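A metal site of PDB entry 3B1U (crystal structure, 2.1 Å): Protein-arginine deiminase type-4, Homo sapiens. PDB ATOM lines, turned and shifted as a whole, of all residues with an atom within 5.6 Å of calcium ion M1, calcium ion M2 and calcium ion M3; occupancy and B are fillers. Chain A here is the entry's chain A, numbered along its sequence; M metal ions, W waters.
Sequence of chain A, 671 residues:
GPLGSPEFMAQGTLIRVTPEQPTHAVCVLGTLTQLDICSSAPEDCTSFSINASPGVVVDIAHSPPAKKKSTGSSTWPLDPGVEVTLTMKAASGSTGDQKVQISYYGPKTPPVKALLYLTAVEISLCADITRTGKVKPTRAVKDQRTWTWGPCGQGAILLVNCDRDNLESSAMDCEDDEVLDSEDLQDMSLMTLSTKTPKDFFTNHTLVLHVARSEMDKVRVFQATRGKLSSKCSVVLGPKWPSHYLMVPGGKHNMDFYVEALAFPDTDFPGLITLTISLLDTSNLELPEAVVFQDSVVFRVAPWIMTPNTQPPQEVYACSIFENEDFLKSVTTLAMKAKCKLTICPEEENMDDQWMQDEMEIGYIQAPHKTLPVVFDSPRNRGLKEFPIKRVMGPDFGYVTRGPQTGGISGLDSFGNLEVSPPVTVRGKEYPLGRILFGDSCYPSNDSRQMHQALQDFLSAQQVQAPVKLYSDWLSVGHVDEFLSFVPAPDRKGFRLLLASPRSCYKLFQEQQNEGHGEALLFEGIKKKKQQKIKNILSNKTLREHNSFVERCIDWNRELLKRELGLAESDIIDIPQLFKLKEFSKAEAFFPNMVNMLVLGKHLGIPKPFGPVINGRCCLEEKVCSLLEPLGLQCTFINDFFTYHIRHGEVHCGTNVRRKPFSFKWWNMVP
Of the 22 residues printed, 3 come within 4 Å of calcium ion M3. The nearest printed residue that does not touch calcium ion M3 is Asp 184 (4.1 Å).
Calcium ion M3 is bound by the backbone carbonyl oxygen of Glu 178, water W3, the backbone carbonyl oxygen of Asp 173, the side-chain carboxylate of Asp 176 and water W2. Calcium ion M3 has five donor atoms within binding distance.
Calcium ion M2 is bound by OD2 of Asp 187, at 2.3 Å. OD2 of Asp 184 binds calcium ion M2 (2.3 Å). Calcium ion M2 is bound by OD1 of Asp 163. Calcium ion M2 is bound by OD1 of Asn 161 (2.4 Å). Calcium ion M2 is bound by OD2 of Asp 165, at 2.4 Å. Calcium ion M2 is bound by OD2 of Asp 173, 2.5 Å away. Calcium ion M2 has six donor atoms within binding distance.
Calcium ion M1 is bound by the side-chain carboxylate (OD1) of Asp 396, water W1, the side-chain carboxylate (OD2) of Asp 163, the side-chain carboxylate (OD2) of Asp 187, the side-chain carboxylate (OD1) of Asp 165, the side-chain carboxylate (OD2) of Asp 165 and the side-chain carboxylate (OD1) of Asp 187.
Water W3 lies within hydrogen-bond range of OD1 of Asp 184 (2.7 Å), OE1 of Glu 260 (2.7 Å) and ND2 of Asn 161 (3.1 Å). Water W2 lies within hydrogen-bond range of the backbone carbonyl oxygen (O) of Asp 176 (2.7 Å) and the side-chain carboxylate (OE2) of Glu 260 (2.7 Å).
Within 4 Å of calcium ion M2: Asn 161, Asp 163, Asp 165, Asp 173, Asp 184 and Asp 187. The nearest printed residue that does not touch calcium ion M2 is Arg 164 (5.1 Å).
Of the 22 residues printed, 4 come within 4 Å of calcium ion M1. The nearest printed residue that does not touch calcium ion M1 is Glu 183 (4.7 Å).
The side-chain amide nitrogen (ND2) of Asn 161 sits at hydrogen-bond distance from the side-chain carboxylate (OE1) of Glu 260 (2.7 Å). O of Asn 161 sits at hydrogen-bond distance from SG of Cys 174, at 3.3 Å.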
ATOM      1  N   ASN A 161     -24.733  16.291  -6.394  1.00  0.00           N
ATOM      2  CA  ASN A 161     -24.838  17.751  -6.309  1.00  0.00           C
ATOM      3  C   ASN A 161     -26.097  18.229  -7.039  1.00  0.00           C
ATOM      4  O   ASN A 161     -26.033  18.910  -8.068  1.00  0.00           O
ATOM      5  CB  ASN A 161     -23.575  18.398  -6.883  1.00  0.00           C
ATOM      6  CG  ASN A 161     -23.430  19.865  -6.507  1.00  0.00           C
ATOM      7  OD1 ASN A 161     -24.217  20.417  -5.733  1.00  0.00           O
ATOM      8  ND2 ASN A 161     -22.414  20.515  -7.064  1.00  0.00           N
ATOM      9  N   ASP A 163     -28.723  20.117  -5.828  1.00  0.00           N
ATOM     10  CA  ASP A 163     -29.337  21.375  -5.421  1.00  0.00           C
ATOM     11  C   ASP A 163     -28.892  22.491  -6.357  1.00  0.00           C
ATOM     12  O   ASP A 163     -28.222  22.238  -7.353  1.00  0.00           O
ATOM     13  CB  ASP A 163     -29.022  21.684  -3.945  1.00  0.00           C
ATOM     14  CG  ASP A 163     -27.580  22.135  -3.733  1.00  0.00           C
ATOM     15  OD1 ASP A 163     -26.704  21.765  -4.531  1.00  0.00           O
ATOM     16  OD2 ASP A 163     -27.333  22.849  -2.735  1.00  0.00           O
ATOM     17  N   ARG A 164     -29.287  23.726  -6.049  1.00  0.00           N
ATOM     18  CA  ARG A 164     -28.968  24.872  -6.892  1.00  0.00           C
ATOM     19  C   ARG A 164     -28.515  26.082  -6.072  1.00  0.00           C
ATOM     20  O   ARG A 164     -29.316  26.951  -5.721  1.00  0.00           O
ATOM     21  CB  ARG A 164     -30.186  25.243  -7.747  1.00  0.00           C
ATOM     22  CG  ARG A 164     -29.907  26.242  -8.847  1.00  0.00           C
ATOM     23  CD  ARG A 164     -31.179  26.536  -9.616  1.00  0.00           C
ATOM     24  NE  ARG A 164     -32.069  27.413  -8.857  1.00  0.00           N
ATOM     25  CZ  ARG A 164     -33.393  27.350  -8.839  1.00  0.00           C
ATOM     26  NH1 ARG A 164     -34.061  26.420  -9.529  1.00  0.00           N
ATOM     27  NH2 ARG A 164     -34.076  28.215  -8.099  1.00  0.00           N
ATOM     28  N   ASP A 165     -27.224  26.118  -5.754  1.00  0.00           N
ATOM     29  CA  ASP A 165     -26.628  27.233  -5.007  1.00  0.00           C
ATOM     30  C   ASP A 165     -26.455  28.465  -5.886  1.00  0.00           C
ATOM     31  O   ASP A 165     -26.456  29.595  -5.392  1.00  0.00           O
ATOM     32  CB  ASP A 165     -25.279  26.830  -4.422  1.00  0.00           C
ATOM     33  CG  ASP A 165     -25.403  25.731  -3.402  1.00  0.00           C
ATOM     34  OD1 ASP A 165     -26.142  25.906  -2.409  1.00  0.00           O
ATOM     35  OD2 ASP A 165     -24.752  24.678  -3.570  1.00  0.00           O
ATOM     36  N   ASP A 173     -26.692  22.287 -10.095  1.00  0.00           N
ATOM     37  CA  ASP A 173     -25.276  22.663 -10.154  1.00  0.00           C
ATOM     38  C   ASP A 173     -24.422  21.648 -10.922  1.00  0.00           C
ATOM     39  O   ASP A 173     -23.424  22.033 -11.544  1.00  0.00           O
ATOM     40  CB  ASP A 173     -24.711  22.853  -8.741  1.00  0.00           C
ATOM     41  CG  ASP A 173     -25.369  24.003  -7.987  1.00  0.00           C
ATOM     42  OD1 ASP A 173     -25.827  24.975  -8.624  1.00  0.00           O
ATOM     43  OD2 ASP A 173     -25.406  23.948  -6.731  1.00  0.00           O
ATOM     44  N   CYS A 174     -24.796  20.367 -10.871  1.00  0.00           N
ATOM     45  CA  CYS A 174     -24.005  19.296 -11.492  1.00  0.00           C
ATOM     46  C   CYS A 174     -24.232  19.108 -13.010  1.00  0.00           C
ATOM     47  O   CYS A 174     -23.606  18.248 -13.622  1.00  0.00           O
ATOM     48  CB  CYS A 174     -24.266  17.970 -10.781  1.00  0.00           C
ATOM     49  SG  CYS A 174     -25.940  17.322 -10.951  1.00  0.00           S
ATOM     50  N   GLU A 175     -25.123  19.903 -13.595  1.00  0.00           N
ATOM     51  CA  GLU A 175     -25.437  19.782 -15.026  1.00  0.00           C
ATOM     52  C   GLU A 175     -24.373  20.409 -15.949  1.00  0.00           C
ATOM     53  O   GLU A 175     -24.314  20.067 -17.127  1.00  0.00           O
ATOM     54  CB  GLU A 175     -26.807  20.394 -15.327  1.00  0.00           C
ATOM     55  CG  GLU A 175     -27.967  19.581 -14.765  1.00  0.00           C
ATOM     56  CD  GLU A 175     -29.329  20.188 -15.093  1.00  0.00           C
ATOM     57  OE1 GLU A 175     -29.526  20.618 -16.248  1.00  0.00           O
ATOM     58  OE2 GLU A 175     -30.200  20.215 -14.197  1.00  0.00           O
ATOM     59  N   ASP A 176     -23.550  21.320 -15.415  1.00  0.00           N
ATOM     60  CA  ASP A 176     -22.443  21.901 -16.177  1.00  0.00           C
ATOM     61  C   ASP A 176     -21.101  21.375 -15.650  1.00  0.00           C
ATOM     62  O   ASP A 176     -21.079  20.564 -14.725  1.00  0.00           O
ATOM     63  CB  ASP A 176     -22.489  23.446 -16.128  1.00  0.00           C
ATOM     64  CG  ASP A 176     -22.190  24.013 -14.754  1.00  0.00           C
ATOM     65  OD1 ASP A 176     -22.226  25.257 -14.611  1.00  0.00           O
ATOM     66  OD2 ASP A 176     -21.920  23.245 -13.801  1.00  0.00           O
ATOM     67  N   ASP A 177     -20.005  21.827 -16.238  1.00  0.00           N
ATOM     68  CA  ASP A 177     -18.662  21.399 -15.815  1.00  0.00           C
ATOM     69  C   ASP A 177     -17.840  22.575 -15.268  1.00  0.00           C
ATOM     70  O   ASP A 177     -16.665  22.747 -15.624  1.00  0.00           O
ATOM     71  CB  ASP A 177     -17.932  20.650 -16.934  1.00  0.00           C
ATOM     72  CG  ASP A 177     -18.104  21.302 -18.292  1.00  0.00           C
ATOM     73  OD1 ASP A 177     -17.495  22.366 -18.530  1.00  0.00           O
ATOM     74  OD2 ASP A 177     -18.846  20.736 -19.129  1.00  0.00           O
ATOM     75  N   GLU A 178     -18.455  23.351 -14.385  1.00  0.00           N
ATOM     76  CA  GLU A 178     -17.805  24.470 -13.701  1.00  0.00           C
ATOM     77  C   GLU A 178     -18.313  24.594 -12.265  1.00  0.00           C
ATOM     78  O   GLU A 178     -19.458  24.256 -11.977  1.00  0.00           O
ATOM     79  CB  GLU A 178     -18.074  25.789 -14.431  1.00  0.00           C
ATOM     80  CG  GLU A 178     -17.694  25.816 -15.901  1.00  0.00           C
ATOM     81  CD  GLU A 178     -17.869  27.191 -16.520  1.00  0.00           C
ATOM     82  OE1 GLU A 178     -17.361  28.175 -15.958  1.00  0.00           O
ATOM     83  OE2 GLU A 178     -18.517  27.279 -17.594  1.00  0.00           O
ATOM     84  N   VAL A 179     -17.451  25.092 -11.375  1.00  0.00           N
ATOM     85  CA  VAL A 179     -17.872  25.467 -10.021  1.00  0.00           C
ATOM     86  C   VAL A 179     -18.169  26.971 -10.022  1.00  0.00           C
ATOM     87  O   VAL A 179     -17.257  27.789  -9.960  1.00  0.00           O
ATOM     88  CB  VAL A 179     -16.785  25.151  -8.977  1.00  0.00           C
ATOM     89  CG1 VAL A 179     -17.232  25.581  -7.587  1.00  0.00           C
ATOM     90  CG2 VAL A 179     -16.445  23.669  -8.991  1.00  0.00           C
ATOM     91  N   LEU A 180     -19.454  27.314 -10.087  1.00  0.00           N
ATOM     92  CA  LEU A 180     -19.886  28.706 -10.248  1.00  0.00           C
ATOM     93  C   LEU A 180     -19.861  29.511  -8.943  1.00  0.00           C
ATOM     94  O   LEU A 180     -19.619  30.718  -8.972  1.00  0.00           O
ATOM     95  CB  LEU A 180     -21.278  28.776 -10.876  1.00  0.00           C
ATOM     96  CG  LEU A 180     -21.368  28.333 -12.343  1.00  0.00           C
ATOM     97  CD1 LEU A 180     -22.824  28.225 -12.779  1.00  0.00           C
ATOM     98  CD2 LEU A 180     -20.600  29.295 -13.245  1.00  0.00           C
ATOM     99  N   GLU A 183     -19.877  28.549  -2.346  1.00  0.00           N
ATOM    100  CA  GLU A 183     -20.761  27.771  -1.466  1.00  0.00           C
ATOM    101  C   GLU A 183     -21.023  26.371  -2.013  1.00  0.00           C
ATOM    102  O   GLU A 183     -21.249  25.432  -1.252  1.00  0.00           O
ATOM    103  CB  GLU A 183     -22.100  28.492  -1.246  1.00  0.00           C
ATOM    104  CG  GLU A 183     -22.016  29.804  -0.470  1.00  0.00           C
ATOM    105  CD  GLU A 183     -21.682  31.014  -1.334  1.00  0.00           C
ATOM    106  OE1 GLU A 183     -21.451  32.105  -0.764  1.00  0.00           O
ATOM    107  OE2 GLU A 183     -21.650  30.889  -2.572  1.00  0.00           O
ATOM    108  N   ASP A 184     -21.005  26.247  -3.338  1.00  0.00           N
ATOM    109  CA  ASP A 184     -21.209  24.972  -4.031  1.00  0.00           C
ATOM    110  C   ASP A 184     -20.185  23.901  -3.603  1.00  0.00           C
ATOM    111  O   ASP A 184     -20.509  22.719  -3.555  1.00  0.00           O
ATOM    112  CB  ASP A 184     -21.150  25.175  -5.549  1.00  0.00           C
ATOM    113  CG  ASP A 184     -21.542  23.928  -6.338  1.00  0.00           C
ATOM    114  OD1 ASP A 184     -20.880  23.635  -7.350  1.00  0.00           O
ATOM    115  OD2 ASP A 184     -22.518  23.249  -5.936  1.00  0.00           O
ATOM    116  N   ASP A 187     -20.933  21.218  -0.834  1.00  0.00           N
ATOM    117  CA  ASP A 187     -21.639  19.987  -1.192  1.00  0.00           C
ATOM    118  C   ASP A 187     -20.715  18.893  -1.708  1.00  0.00           C
ATOM    119  O   ASP A 187     -21.120  17.732  -1.774  1.00  0.00           O
ATOM    120  CB  ASP A 187     -22.689  20.281  -2.260  1.00  0.00           C
ATOM    121  CG  ASP A 187     -23.759  21.229  -1.788  1.00  0.00           C
ATOM    122  OD1 ASP A 187     -24.073  21.256  -0.583  1.00  0.00           O
ATOM    123  OD2 ASP A 187     -24.295  21.970  -2.639  1.00  0.00           O
ATOM    124  N   MET A 188     -19.492  19.250  -2.072  1.00  0.00           N
ATOM    125  CA  MET A 188     -18.558  18.309  -2.702  1.00  0.00           C
ATOM    126  C   MET A 188     -17.648  17.647  -1.685  1.00  0.00           C
ATOM    127  O   MET A 188     -17.434  18.176  -0.591  1.00  0.00           O
ATOM    128  CB  MET A 188     -17.729  19.044  -3.759  1.00  0.00           C
ATOM    129  CG  MET A 188     -18.574  19.708  -4.833  1.00  0.00           C
ATOM    130  SD  MET A 188     -17.596  20.308  -6.217  1.00  0.00           S
ATOM    131  CE  MET A 188     -18.798  21.337  -7.047  1.00  0.00           C
ATOM    132  N   PHE A 222     -13.013  18.371  -9.758  1.00  0.00           N
ATOM    133  CA  PHE A 222     -12.398  19.676  -9.997  1.00  0.00           C
ATOM    134  C   PHE A 222     -11.072  19.771  -9.254  1.00  0.00           C
ATOM    135  O   PHE A 222     -10.945  19.250  -8.142  1.00  0.00           O
ATOM    136  CB  PHE A 222     -13.309  20.806  -9.515  1.00  0.00           C
ATOM    137  CG  PHE A 222     -14.647  20.847 -10.210  1.00  0.00           C
ATOM    138  CD1 PHE A 222     -15.727  20.151  -9.688  1.00  0.00           C
ATOM    139  CD2 PHE A 222     -14.818  21.579 -11.378  1.00  0.00           C
ATOM    140  CE1 PHE A 222     -16.964  20.183 -10.318  1.00  0.00           C
ATOM    141  CE2 PHE A 222     -16.046  21.614 -12.010  1.00  0.00           C
ATOM    142  CZ  PHE A 222     -17.117  20.922 -11.489  1.00  0.00           C
ATOM    143  N   GLU A 260     -17.929  15.727  -7.071  1.00  0.00           N
ATOM    144  CA  GLU A 260     -19.394  15.710  -7.017  1.00  0.00           C
ATOM    145  C   GLU A 260     -19.933  14.501  -7.760  1.00  0.00           C
ATOM    146  O   GLU A 260     -19.358  14.091  -8.776  1.00  0.00           O
ATOM    147  CB  GLU A 260     -19.976  16.996  -7.620  1.00  0.00           C
ATOM    148  CG  GLU A 260     -19.590  17.244  -9.077  1.00  0.00           C
ATOM    149  CD  GLU A 260     -20.240  18.478  -9.684  1.00  0.00           C
ATOM    150  OE1 GLU A 260     -20.785  19.306  -8.916  1.00  0.00           O
ATOM    151  OE2 GLU A 260     -20.209  18.615 -10.921  1.00  0.00           O
ATOM    152  N   LYS A 370     -21.763  17.338   4.874  1.00  0.00           N
ATOM    153  CA  LYS A 370     -22.938  18.083   4.420  1.00  0.00           C
ATOM    154  C   LYS A 370     -24.208  17.227   4.393  1.00  0.00           C
ATOM    155  O   LYS A 370     -24.201  16.076   3.956  1.00  0.00           O
ATOM    156  CB  LYS A 370     -22.668  18.666   3.027  1.00  0.00           C
ATOM    157  CG  LYS A 370     -23.839  19.405   2.382  1.00  0.00           C
ATOM    158  CD  LYS A 370     -24.199  20.699   3.115  1.00  0.00           C
ATOM    159  CE  LYS A 370     -23.205  21.807   2.825  1.00  0.00           C
ATOM    160  NZ  LYS A 370     -23.622  23.108   3.418  1.00  0.00           N
ATOM    161  N   LEU A 372     -28.391  17.890   3.258  1.00  0.00           N
ATOM    162  CA  LEU A 372     -29.395  18.795   2.695  1.00  0.00           C
ATOM    163  C   LEU A 372     -30.683  18.067   2.317  1.00  0.00           C
ATOM    164  O   LEU A 372     -30.646  16.895   1.953  1.00  0.00           O
ATOM    165  CB  LEU A 372     -28.843  19.529   1.465  1.00  0.00           C
ATOM    166  CG  LEU A 372     -28.292  18.693   0.307  1.00  0.00           C
ATOM    167  CD1 LEU A 372     -28.503  19.397  -1.036  1.00  0.00           C
ATOM    168  CD2 LEU A 372     -26.820  18.377   0.519  1.00  0.00           C
ATOM    169  N   PRO A 395     -31.080  26.772  -3.196  1.00  0.00           N
ATOM    170  CA  PRO A 395     -29.893  26.718  -2.326  1.00  0.00           C
ATOM    171  C   PRO A 395     -30.052  25.741  -1.164  1.00  0.00           C
ATOM    172  O   PRO A 395     -30.933  25.915  -0.321  1.00  0.00           O
ATOM    173  CB  PRO A 395     -29.777  28.171  -1.819  1.00  0.00           C
ATOM    174  CG  PRO A 395     -30.418  28.991  -2.875  1.00  0.00           C
ATOM    175  CD  PRO A 395     -31.538  28.153  -3.411  1.00  0.00           C
ATOM    176  N   ASP A 396     -29.198  24.717  -1.144  1.00  0.00           N
ATOM    177  CA  ASP A 396     -29.267  23.635  -0.146  1.00  0.00           C
ATOM    178  C   ASP A 396     -30.624  22.911  -0.136  1.00  0.00           C
ATOM    179  O   ASP A 396     -31.079  22.443   0.911  1.00  0.00           O
ATOM    180  CB  ASP A 396     -28.910  24.150   1.265  1.00  0.00           C
ATOM    181  CG  ASP A 396     -27.454  24.578   1.380  1.00  0.00           C
ATOM    182  OD1 ASP A 396     -26.602  24.038   0.636  1.00  0.00           O
ATOM    183  OD2 ASP A 396     -27.146  25.459   2.205  1.00  0.00           O
HETATM  184 CA    CA M   1     -25.530  23.612  -1.294  1.00  0.00          CA
HETATM  185 CA    CA M   2     -24.492  22.640  -4.854  1.00  0.00          CA
HETATM  186 CA    CA M   3     -21.406  23.174 -11.437  1.00  0.00          CA
HETATM  187  O   HOH W   1     -23.886  25.020  -0.602  1.00  0.00           O
HETATM  188  O   HOH W   2     -20.536  21.017 -12.162  1.00  0.00           O
HETATM  189  O   HOH W   3     -21.053  21.972  -9.502  1.00  0.00           O
